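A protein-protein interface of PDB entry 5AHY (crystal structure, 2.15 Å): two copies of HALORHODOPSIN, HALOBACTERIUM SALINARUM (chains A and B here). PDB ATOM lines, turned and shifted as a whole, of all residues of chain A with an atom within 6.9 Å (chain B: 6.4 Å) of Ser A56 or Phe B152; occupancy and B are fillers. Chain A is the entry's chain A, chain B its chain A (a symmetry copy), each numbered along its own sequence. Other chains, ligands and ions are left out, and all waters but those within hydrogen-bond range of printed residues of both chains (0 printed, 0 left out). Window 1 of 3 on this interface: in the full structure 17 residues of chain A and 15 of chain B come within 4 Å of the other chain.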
ATOM      1  N   ALA A  21      12.358  24.407   4.178  1.00  0.00           N
ATOM      2  CA  ALA A  21      11.755  25.168   3.089  1.00  0.00           C
ATOM      3  C   ALA A  21      10.917  24.226   2.209  1.00  0.00           C
ATOM      4  O   ALA A  21       9.822  24.582   1.773  1.00  0.00           O
ATOM      5  CB  ALA A  21      12.828  25.893   2.251  1.00  0.00           C
ATOM      6  N   LEU A  48       3.933  32.071  -0.992  1.00  0.00           N
ATOM      7  CA  LEU A  48       4.478  30.794  -1.449  1.00  0.00           C
ATOM      8  C   LEU A  48       5.849  30.937  -2.123  1.00  0.00           C
ATOM      9  O   LEU A  48       6.664  30.015  -2.104  1.00  0.00           O
ATOM     10  CB  LEU A  48       3.487  30.138  -2.416  1.00  0.00           C
ATOM     11  CG  LEU A  48       3.918  28.860  -3.126  1.00  0.00           C
ATOM     12  CD1 LEU A  48       4.120  27.738  -2.102  1.00  0.00           C
ATOM     13  CD2 LEU A  48       2.874  28.482  -4.194  1.00  0.00           C
ATOM     14  N   MET A  49       6.092  32.098  -2.724  1.00  0.00           N
ATOM     15  CA  MET A  49       7.378  32.384  -3.369  1.00  0.00           C
ATOM     16  C   MET A  49       8.537  32.384  -2.367  1.00  0.00           C
ATOM     17  O   MET A  49       9.673  32.050  -2.703  1.00  0.00           O
ATOM     18  CB  MET A  49       7.308  33.733  -4.082  1.00  0.00           C
ATOM     19  CG  MET A  49       6.413  33.721  -5.311  1.00  0.00           C
ATOM     20  SD  MET A  49       7.210  32.773  -6.615  1.00  0.00           S
ATOM     21  CE  MET A  49       8.780  33.643  -6.664  1.00  0.00           C
ATOM     22  N   PRO A  51       9.420  30.508   0.454  1.00  0.00           N
ATOM     23  CA  PRO A  51      10.274  29.319   0.584  1.00  0.00           C
ATOM     24  C   PRO A  51      10.732  28.731  -0.749  1.00  0.00           C
ATOM     25  O   PRO A  51      11.720  27.987  -0.759  1.00  0.00           O
ATOM     26  CB  PRO A  51       9.390  28.320   1.337  1.00  0.00           C
ATOM     27  CG  PRO A  51       7.974  28.740   1.043  1.00  0.00           C
ATOM     28  CD  PRO A  51       8.026  30.243   0.881  1.00  0.00           C
ATOM     29  N   LEU A  52      10.041  29.033  -1.846  1.00  0.00           N
ATOM     30  CA  LEU A  52      10.543  28.608  -3.151  1.00  0.00           C
ATOM     31  C   LEU A  52      11.919  29.213  -3.422  1.00  0.00           C
ATOM     32  O   LEU A  52      12.828  28.520  -3.874  1.00  0.00           O
ATOM     33  CB  LEU A  52       9.570  28.985  -4.268  1.00  0.00           C
ATOM     34  CG  LEU A  52       8.494  27.907  -4.481  1.00  0.00           C
ATOM     35  CD1 LEU A  52       7.425  28.397  -5.459  1.00  0.00           C
ATOM     36  CD2 LEU A  52       9.145  26.603  -4.974  1.00  0.00           C
ATOM     37  N   VAL A  53      12.081  30.501  -3.153  1.00  0.00           N
ATOM     38  CA  VAL A  53      13.394  31.132  -3.356  1.00  0.00           C
ATOM     39  C   VAL A  53      14.394  30.637  -2.319  1.00  0.00           C
ATOM     40  O   VAL A  53      15.572  30.387  -2.629  1.00  0.00           O
ATOM     41  CB  VAL A  53      13.308  32.667  -3.289  1.00  0.00           C
ATOM     42  CG1 VAL A  53      14.715  33.295  -3.408  1.00  0.00           C
ATOM     43  CG2 VAL A  53      12.351  33.178  -4.384  1.00  0.00           C
ATOM     44  N   SER A  54      13.917  30.487  -1.087  1.00  0.00           N
ATOM     45  CA  SER A  54      14.779  30.034  -0.005  1.00  0.00           C
ATOM     46  C   SER A  54      15.391  28.670  -0.310  1.00  0.00           C
ATOM     47  O   SER A  54      16.599  28.496  -0.167  1.00  0.00           O
ATOM     48  CB  SER A  54      14.016  29.976   1.327  1.00  0.00           C
ATOM     49  OG  SER A  54      14.909  29.700   2.387  1.00  0.00           O
ATOM     50  N   ILE A  55      14.581  27.699  -0.741  1.00  0.00           N
ATOM     51  CA  ILE A  55      15.155  26.374  -0.972  1.00  0.00           C
ATOM     52  C   ILE A  55      16.187  26.413  -2.122  1.00  0.00           C
ATOM     53  O   ILE A  55      17.162  25.661  -2.108  1.00  0.00           O
ATOM     54  CB  ILE A  55      14.066  25.298  -1.262  1.00  0.00           C
ATOM     55  CG1 ILE A  55      14.670  23.892  -1.155  1.00  0.00           C
ATOM     56  CG2 ILE A  55      13.414  25.500  -2.653  1.00  0.00           C
ATOM     57  CD1 ILE A  55      13.600  22.744  -1.107  1.00  0.00           C
ATOM     58  N   SER A  56      15.984  27.315  -3.084  1.00  0.00           N
ATOM     59  CA  SER A  56      16.914  27.512  -4.204  1.00  0.00           C
ATOM     60  C   SER A  56      18.259  27.999  -3.710  1.00  0.00           C
ATOM     61  O   SER A  56      19.324  27.567  -4.169  1.00  0.00           O
ATOM     62  CB  SER A  56      16.351  28.531  -5.199  1.00  0.00           C
ATOM     63  OG  SER A  56      15.060  28.148  -5.640  1.00  0.00           O
ATOM     64  N   SER A  57      18.182  28.915  -2.758  1.00  0.00           N
ATOM     65  CA  SER A  57      19.345  29.521  -2.157  1.00  0.00           C
ATOM     66  C   SER A  57      20.175  28.469  -1.461  1.00  0.00           C
ATOM     67  O   SER A  57      21.379  28.398  -1.645  1.00  0.00           O
ATOM     68  CB  SER A  57      18.915  30.609  -1.170  1.00  0.00           C
ATOM     69  OG  SER A  57      20.052  31.295  -0.701  1.00  0.00           O
ATOM     70  N   TYR A  58      19.519  27.615  -0.682  1.00  0.00           N
ATOM     71  CA  TYR A  58      20.246  26.611   0.082  1.00  0.00           C
ATOM     72  C   TYR A  58      20.863  25.553  -0.829  1.00  0.00           C
ATOM     73  O   TYR A  58      21.921  25.034  -0.523  1.00  0.00           O
ATOM     74  CB  TYR A  58      19.332  25.972   1.152  1.00  0.00           C
ATOM     75  CG  TYR A  58      19.228  26.874   2.374  1.00  0.00           C
ATOM     76  CD1 TYR A  58      20.271  26.927   3.312  1.00  0.00           C
ATOM     77  CD2 TYR A  58      18.132  27.722   2.559  1.00  0.00           C
ATOM     78  CE1 TYR A  58      20.210  27.777   4.424  1.00  0.00           C
ATOM     79  CE2 TYR A  58      18.066  28.587   3.673  1.00  0.00           C
ATOM     80  CZ  TYR A  58      19.109  28.599   4.596  1.00  0.00           C
ATOM     81  OH  TYR A  58      19.052  29.421   5.698  1.00  0.00           O
ATOM     82  N   LEU A  59      20.216  25.234  -1.944  1.00  0.00           N
ATOM     83  CA  LEU A  59      20.847  24.331  -2.907  1.00  0.00           C
ATOM     84  C   LEU A  59      22.046  25.023  -3.577  1.00  0.00           C
ATOM     85  O   LEU A  59      23.049  24.386  -3.877  1.00  0.00           O
ATOM     86  CB  LEU A  59      19.847  23.871  -3.961  1.00  0.00           C
ATOM     87  CG  LEU A  59      18.703  22.993  -3.440  1.00  0.00           C
ATOM     88  CD1 LEU A  59      17.552  23.054  -4.420  1.00  0.00           C
ATOM     89  CD2 LEU A  59      19.168  21.542  -3.229  1.00  0.00           C
ATOM     90  N   GLY A  60      21.929  26.329  -3.809  1.00  0.00           N
ATOM     91  CA  GLY A  60      23.047  27.116  -4.304  1.00  0.00           C
ATOM     92  C   GLY A  60      24.259  26.963  -3.403  1.00  0.00           C
ATOM     93  O   GLY A  60      25.371  26.721  -3.883  1.00  0.00           O
ATOM     94  N   LEU A  61      24.041  27.071  -2.090  1.00  0.00           N
ATOM     95  CA  LEU A  61      25.138  26.957  -1.130  1.00  0.00           C
ATOM     96  C   LEU A  61      25.663  25.526  -1.021  1.00  0.00           C
ATOM     97  O   LEU A  61      26.873  25.305  -1.009  1.00  0.00           O
ATOM     98  CB  LEU A  61      24.697  27.463   0.249  1.00  0.00           C
ATOM     99  CG  LEU A  61      24.226  28.920   0.331  1.00  0.00           C
ATOM    100  CD1 LEU A  61      23.566  29.219   1.679  1.00  0.00           C
ATOM    101  CD2 LEU A  61      25.384  29.883   0.092  1.00  0.00           C
ATOM    102  N   THR A  66      27.384  28.884  -5.013  1.00  0.00           N
ATOM    103  CA  THR A  66      27.332  30.259  -4.506  1.00  0.00           C
ATOM    104  C   THR A  66      28.074  30.432  -3.184  1.00  0.00           C
ATOM    105  O   THR A  66      27.686  31.249  -2.343  1.00  0.00           O
ATOM    106  CB  THR A  66      25.880  30.739  -4.316  1.00  0.00           C
ATOM    107  OG1 THR A  66      25.219  29.915  -3.341  1.00  0.00           O
ATOM    108  CG2 THR A  66      25.112  30.697  -5.628  1.00  0.00           C
ATOM    109  N   THR A  92      20.445  35.821  -3.013  1.00  0.00           N
ATOM    110  CA  THR A  92      19.059  35.388  -3.128  1.00  0.00           C
ATOM    111  C   THR A  92      18.158  36.213  -2.232  1.00  0.00           C
ATOM    112  O   THR A  92      16.956  36.279  -2.448  1.00  0.00           O
ATOM    113  CB  THR A  92      18.911  33.876  -2.811  1.00  0.00           C
ATOM    114  OG1 THR A  92      19.361  33.617  -1.480  1.00  0.00           O
ATOM    115  CG2 THR A  92      19.780  33.062  -3.779  1.00  0.00           C
ATOM    116  N   LEU A  95      16.032  38.586  -4.052  1.00  0.00           N
ATOM    117  CA  LEU A  95      14.757  38.108  -4.600  1.00  0.00           C
ATOM    118  C   LEU A  95      13.761  37.659  -3.519  1.00  0.00           C
ATOM    119  O   LEU A  95      12.576  37.895  -3.658  1.00  0.00           O
ATOM    120  CB  LEU A  95      14.990  36.953  -5.587  1.00  0.00           C
ATOM    121  CG  LEU A  95      13.736  36.274  -6.147  1.00  0.00           C
ATOM    122  CD1 LEU A  95      12.767  37.305  -6.741  1.00  0.00           C
ATOM    123  CD2 LEU A  95      14.107  35.215  -7.190  1.00  0.00           C
ATOM    124  N   VAL B 118       3.621  36.574 -10.600  1.00  0.00           N
ATOM    125  CA  VAL B 118       3.945  35.798 -11.797  1.00  0.00           C
ATOM    126  C   VAL B 118       5.327  36.158 -12.325  1.00  0.00           C
ATOM    127  O   VAL B 118       6.137  35.276 -12.614  1.00  0.00           O
ATOM    128  CB  VAL B 118       2.903  36.011 -12.915  1.00  0.00           C
ATOM    129  CG1 VAL B 118       3.342  35.321 -14.197  1.00  0.00           C
ATOM    130  CG2 VAL B 118       1.543  35.492 -12.469  1.00  0.00           C
ATOM    131  N   ALA B 120       7.756  37.462 -10.744  1.00  0.00           N
ATOM    132  CA  ALA B 120       8.754  36.989  -9.787  1.00  0.00           C
ATOM    133  C   ALA B 120       8.976  35.473  -9.923  1.00  0.00           C
ATOM    134  O   ALA B 120      10.109  35.011  -9.877  1.00  0.00           O
ATOM    135  CB  ALA B 120       8.348  37.351  -8.336  1.00  0.00           C
ATOM    136  N   ALA B 121       7.899  34.702 -10.086  1.00  0.00           N
ATOM    137  CA  ALA B 121       8.051  33.266 -10.317  1.00  0.00           C
ATOM    138  C   ALA B 121       8.840  33.011 -11.577  1.00  0.00           C
ATOM    139  O   ALA B 121       9.714  32.135 -11.623  1.00  0.00           O
ATOM    140  CB  ALA B 121       6.690  32.579 -10.407  1.00  0.00           C
ATOM    141  N   ASP B 122       8.520  33.788 -12.606  1.00  0.00           N
ATOM    142  CA  ASP B 122       9.157  33.640 -13.900  1.00  0.00           C
ATOM    143  C   ASP B 122      10.668  33.849 -13.789  1.00  0.00           C
ATOM    144  O   ASP B 122      11.457  33.092 -14.359  1.00  0.00           O
ATOM    145  CB  ASP B 122       8.555  34.622 -14.905  1.00  0.00           C
ATOM    146  CG  ASP B 122       9.246  34.558 -16.243  1.00  0.00           C
ATOM    147  OD1 ASP B 122       8.899  33.673 -17.050  1.00  0.00           O
ATOM    148  OD2 ASP B 122      10.159  35.373 -16.473  1.00  0.00           O
ATOM    149  N   ILE B 123      11.068  34.873 -13.040  1.00  0.00           N
ATOM    150  CA  ILE B 123      12.489  35.141 -12.842  1.00  0.00           C
ATOM    151  C   ILE B 123      13.149  34.010 -12.045  1.00  0.00           C
ATOM    152  O   ILE B 123      14.246  33.574 -12.382  1.00  0.00           O
ATOM    153  CB  ILE B 123      12.711  36.500 -12.142  1.00  0.00           C
ATOM    154  CG1 ILE B 123      12.291  37.650 -13.074  1.00  0.00           C
ATOM    155  CG2 ILE B 123      14.178  36.677 -11.732  1.00  0.00           C
ATOM    156  CD1 ILE B 123      12.204  39.005 -12.349  1.00  0.00           C
ATOM    157  N   GLY B 124      12.480  33.531 -11.001  1.00  0.00           N
ATOM    158  CA  GLY B 124      12.963  32.362 -10.274  1.00  0.00           C
ATOM    159  C   GLY B 124      13.194  31.153 -11.186  1.00  0.00           C
ATOM    160  O   GLY B 124      14.198  30.456 -11.052  1.00  0.00           O
ATOM    161  N   MET B 125      12.249  30.907 -12.094  1.00  0.00           N
ATOM    162  CA  MET B 125      12.358  29.832 -13.088  1.00  0.00           C
ATOM    163  C   MET B 125      13.654  29.964 -13.884  1.00  0.00           C
ATOM    164  O   MET B 125      14.391  28.999 -14.047  1.00  0.00           O
ATOM    165  CB  MET B 125      11.146  29.855 -14.048  1.00  0.00           C
ATOM    166  CG  MET B 125      11.103  28.726 -15.095  1.00  0.00           C
ATOM    167  SD  MET B 125       9.779  28.914 -16.337  1.00  0.00           S
ATOM    168  CE  MET B 125      10.377  30.373 -17.203  1.00  0.00           C
ATOM    169  N   CYS B 126      13.921  31.179 -14.363  1.00  0.00           N
ATOM    170  CA  CYS B 126      15.058  31.418 -15.235  1.00  0.00           C
ATOM    171  C   CYS B 126      16.364  31.275 -14.464  1.00  0.00           C
ATOM    172  O   CYS B 126      17.294  30.653 -14.956  1.00  0.00           O
ATOM    173  CB  CYS B 126      14.955  32.807 -15.895  1.00  0.00           C
ATOM    174  SG  CYS B 126      13.531  32.930 -17.041  1.00  0.00           S
ATOM    175  N   THR B 128      16.997  29.609 -11.636  1.00  0.00           N
ATOM    176  CA  THR B 128      17.284  28.251 -11.158  1.00  0.00           C
ATOM    177  C   THR B 128      17.651  27.335 -12.350  1.00  0.00           C
ATOM    178  O   THR B 128      18.498  26.455 -12.228  1.00  0.00           O
ATOM    179  CB  THR B 128      16.114  27.679 -10.301  1.00  0.00           C
ATOM    180  OG1 THR B 128      14.867  27.740 -11.010  1.00  0.00           O
ATOM    181  CG2 THR B 128      15.977  28.502  -9.035  1.00  0.00           C
ATOM    182  N   PHE B 145      17.919  21.628  -9.054  1.00  0.00           N
ATOM    183  CA  PHE B 145      17.655  22.967  -9.602  1.00  0.00           C
ATOM    184  C   PHE B 145      16.628  22.915 -10.734  1.00  0.00           C
ATOM    185  O   PHE B 145      15.726  23.760 -10.800  1.00  0.00           O
ATOM    186  CB  PHE B 145      18.956  23.623 -10.099  1.00  0.00           C
ATOM    187  CG  PHE B 145      19.730  24.327  -9.021  1.00  0.00           C
ATOM    188  CD1 PHE B 145      19.103  25.257  -8.198  1.00  0.00           C
ATOM    189  CD2 PHE B 145      21.075  24.054  -8.820  1.00  0.00           C
ATOM    190  CE1 PHE B 145      19.803  25.911  -7.191  1.00  0.00           C
ATOM    191  CE2 PHE B 145      21.791  24.698  -7.807  1.00  0.00           C
ATOM    192  CZ  PHE B 145      21.151  25.632  -6.995  1.00  0.00           C
ATOM    193  N   ALA B 147      14.214  20.737 -11.029  1.00  0.00           N
ATOM    194  CA  ALA B 147      12.899  20.508 -10.408  1.00  0.00           C
ATOM    195  C   ALA B 147      12.305  21.774  -9.769  1.00  0.00           C
ATOM    196  O   ALA B 147      11.101  22.013  -9.848  1.00  0.00           O
ATOM    197  CB  ALA B 147      12.998  19.391  -9.354  1.00  0.00           C
ATOM    198  N   ILE B 148      13.142  22.571  -9.115  1.00  0.00           N
ATOM    199  CA  ILE B 148      12.689  23.855  -8.564  1.00  0.00           C
ATOM    200  C   ILE B 148      12.257  24.799  -9.680  1.00  0.00           C
ATOM    201  O   ILE B 148      11.228  25.467  -9.573  1.00  0.00           O
ATOM    202  CB  ILE B 148      13.785  24.556  -7.732  1.00  0.00           C
ATOM    203  CG1 ILE B 148      14.263  23.624  -6.634  1.00  0.00           C
ATOM    204  CG2 ILE B 148      13.214  25.843  -7.077  1.00  0.00           C
ATOM    205  CD1 ILE B 148      13.119  23.132  -5.802  1.00  0.00           C
ATOM    206  N   SER B 149      13.055  24.845 -10.747  1.00  0.00           N
ATOM    207  CA  SER B 149      12.701  25.634 -11.927  1.00  0.00           C
ATOM    208  C   SER B 149      11.314  25.244 -12.443  1.00  0.00           C
ATOM    209  O   SER B 149      10.486  26.115 -12.729  1.00  0.00           O
ATOM    210  CB  SER B 149      13.755  25.453 -13.022  1.00  0.00           C
ATOM    211  OG  SER B 149      13.608  26.425 -14.045  1.00  0.00           O
ATOM    212  N   CYS B 150      11.060  23.936 -12.541  1.00  0.00           N
ATOM    213  CA  CYS B 150       9.723  23.431 -12.888  1.00  0.00           C
ATOM    214  C   CYS B 150       8.613  23.914 -11.957  1.00  0.00           C
ATOM    215  O   CYS B 150       7.506  24.224 -12.411  1.00  0.00           O
ATOM    216  CB  CYS B 150       9.729  21.892 -12.904  1.00  0.00           C
ATOM    217  SG  CYS B 150      10.629  21.200 -14.309  1.00  0.00           S
ATOM    218  N   ALA B 151       8.895  23.941 -10.653  1.00  0.00           N
ATOM    219  CA  ALA B 151       7.933  24.432  -9.668  1.00  0.00           C
ATOM    220  C   ALA B 151       7.613  25.904  -9.912  1.00  0.00           C
ATOM    221  O   ALA B 151       6.459  26.316  -9.808  1.00  0.00           O
ATOM    222  CB  ALA B 151       8.466  24.228  -8.233  1.00  0.00           C
ATOM    223  N   PHE B 152       8.633  26.699 -10.239  1.00  0.00           N
ATOM    224  CA  PHE B 152       8.407  28.102 -10.587  1.00  0.00           C
ATOM    225  C   PHE B 152       7.548  28.195 -11.847  1.00  0.00           C
ATOM    226  O   PHE B 152       6.618  28.995 -11.911  1.00  0.00           O
ATOM    227  CB  PHE B 152       9.731  28.845 -10.805  1.00  0.00           C
ATOM    228  CG  PHE B 152      10.406  29.300  -9.539  1.00  0.00           C
ATOM    229  CD1 PHE B 152       9.756  30.156  -8.654  1.00  0.00           C
ATOM    230  CD2 PHE B 152      11.710  28.913  -9.257  1.00  0.00           C
ATOM    231  CE1 PHE B 152      10.383  30.606  -7.496  1.00  0.00           C
ATOM    232  CE2 PHE B 152      12.350  29.363  -8.096  1.00  0.00           C
ATOM    233  CZ  PHE B 152      11.677  30.207  -7.214  1.00  0.00           C
ATOM    234  N   PHE B 153       7.864  27.363 -12.841  1.00  0.00           N
ATOM    235  CA  PHE B 153       7.117  27.291 -14.110  1.00  0.00           C
ATOM    236  C   PHE B 153       5.620  26.993 -13.858  1.00  0.00           C
ATOM    237  O   PHE B 153       4.728  27.608 -14.458  1.00  0.00           O
ATOM    238  CB  PHE B 153       7.742  26.206 -15.019  1.00  0.00           C
ATOM    239  CG  PHE B 153       7.208  26.178 -16.444  1.00  0.00           C
ATOM    240  CD1 PHE B 153       6.539  27.267 -16.992  1.00  0.00           C
ATOM    241  CD2 PHE B 153       7.387  25.040 -17.240  1.00  0.00           C
ATOM    242  CE1 PHE B 153       6.062  27.228 -18.311  1.00  0.00           C
ATOM    243  CE2 PHE B 153       6.914  24.995 -18.558  1.00  0.00           C
ATOM    244  CZ  PHE B 153       6.247  26.089 -19.094  1.00  0.00           C
ATOM    245  N   VAL B 154       5.359  26.044 -12.968  1.00  0.00           N
ATOM    246  CA  VAL B 154       3.992  25.684 -12.602  1.00  0.00           C
ATOM    247  C   VAL B 154       3.221  26.863 -11.992  1.00  0.00           C
ATOM    248  O   VAL B 154       2.052  27.073 -12.311  1.00  0.00           O
ATOM    249  CB  VAL B 154       3.989  24.502 -11.618  1.00  0.00           C
ATOM    250  CG1 VAL B 154       2.596  24.285 -11.051  1.00  0.00           C
ATOM    251  CG2 VAL B 154       4.514  23.235 -12.310  1.00  0.00           C
ATOM    252  N   VAL B 155       3.881  27.639 -11.132  1.00  0.00           N
ATOM    253  CA  VAL B 155       3.286  28.867 -10.594  1.00  0.00           C
ATOM    254  C   VAL B 155       2.829  29.801 -11.718  1.00  0.00           C
ATOM    255  O   VAL B 155       1.683  30.262 -11.728  1.00  0.00           O
ATOM    256  CB  VAL B 155       4.270  29.632  -9.673  1.00  0.00           C
ATOM    257  CG1 VAL B 155       3.702  30.997  -9.306  1.00  0.00           C
ATOM    258  CG2 VAL B 155       4.558  28.828  -8.411  1.00  0.00           C
ATOM    259  N   VAL B 156       3.729  30.078 -12.658  1.00  0.00           N
ATOM    260  CA  VAL B 156       3.404  30.898 -13.823  1.00  0.00           C
ATOM    261  C   VAL B 156       2.224  30.319 -14.627  1.00  0.00           C
ATOM    262  O   VAL B 156       1.239  31.010 -14.849  1.00  0.00           O
ATOM    263  CB  VAL B 156       4.620  31.062 -14.743  1.00  0.00           C
ATOM    264  CG1 VAL B 156       4.201  31.682 -16.082  1.00  0.00           C
ATOM    265  CG2 VAL B 156       5.682  31.921 -14.050  1.00  0.00           C
ATOM    266  N   LEU B 157       2.326  29.054 -15.033  1.00  0.00           N
ATOM    267  CA  LEU B 157       1.271  28.368 -15.794  1.00  0.00           C
ATOM    268  C   LEU B 157      -0.102  28.380 -15.111  1.00  0.00           C
ATOM    269  O   LEU B 157      -1.130  28.639 -15.745  1.00  0.00           O
ATOM    270  CB  LEU B 157       1.670  26.911 -16.039  1.00  0.00           C
ATOM    271  CG  LEU B 157       2.830  26.563 -16.958  1.00  0.00           C
ATOM    272  CD1 LEU B 157       3.101  25.067 -16.893  1.00  0.00           C
ATOM    273  CD2 LEU B 157       2.532  26.992 -18.376  1.00  0.00           C
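OG of Ser A56 is in hydrogen-bond range of O of Leu A52 (2.9 Å).
O of Gly A60 sits at hydrogen-bond distance from N of Thr A66, at 3.2 Å.
The backbone carbonyl oxygen of Gly B124 sits at hydrogen-bond distance from the side-chain hydroxyl of Thr B128 (2.8 Å).
The backbone carbonyl oxygen of Met B125 lies within hydrogen-bond range of the side-chain hydroxyl of Thr B128, at 3.3 Å.
The side-chain hydroxyl of Thr B128 sits close to the backbone NH of Ser B149, 3.4 Å away.
Among the printed residues, merely in contact across the chains: Met A49 with Ala B120 (3.7 Å), Met A49 with Ala B121 (3.7 Å), Met A49 with Phe B152 (3.5 Å), Leu A52 with Phe B152 (3.7 Å), Ile A55 with Ile B148 (3.95 Å), Ser A56 with Thr B128 (3.5 Å), Ser A56 with Phe B145 (3.5 Å), Ser A56 with Ile B148 (3.3 Å), Ser A56 with Phe B152 (3.9 Å), Leu A59 with Phe B145 (3.6 Å) and Gly A60 with Phe B145 (3.4 Å).
Of chain B, only Thr B128 (3.5 Å), Phe B145 (3.5 Å), Ile B148 (3.3 Å) and Phe B152 (3.9 Å) come within 4 Å of Ser A56.
Of the printed residues of chain A, Phe B152 touches Met A49, Leu A52 and Ser A56.
Of the printed residues of chain A, Ile B148 touches Ile A55 and Ser A56.
Printed residues of chain A within 4 Å of Ala B120: Met A49.
Printed residues of chain B within 4 Å of Ile A55: Ile B148.
Of the printed residues of chain A, Thr B128 touches Ser A56.
Met B125 touches none of the printed residues of chain A.
The nearest residue of chain B that does not touch Ser A56 is Gly B124 (5.9 Å).
The nearest residue of chain A that does not touch Phe B152 is Val A53 (4.1 Å).
The nearest printed residue of chain B that does not touch Met A49 is Val B155 (4.8 Å).
Printed residues of chain B that touch a printed residue of chain A: Ala B120, Ala B121, Thr B128, Phe B145, Ile B148 and Phe B152.
Along chain B the printed residues that touch a printed residue of chain A span positions 120 to 152.
Hydrophobic or aromatic side chains of chain A within 4 Å of the printed part of chain B: Met A49, Leu A52, Ile A55 and Leu A59.
Among the printed residues, no Asp or Glu carboxylate lies within 4 Å of a Lys or Arg side-chain nitrogen of the other chain.
No position is printed for both chains.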
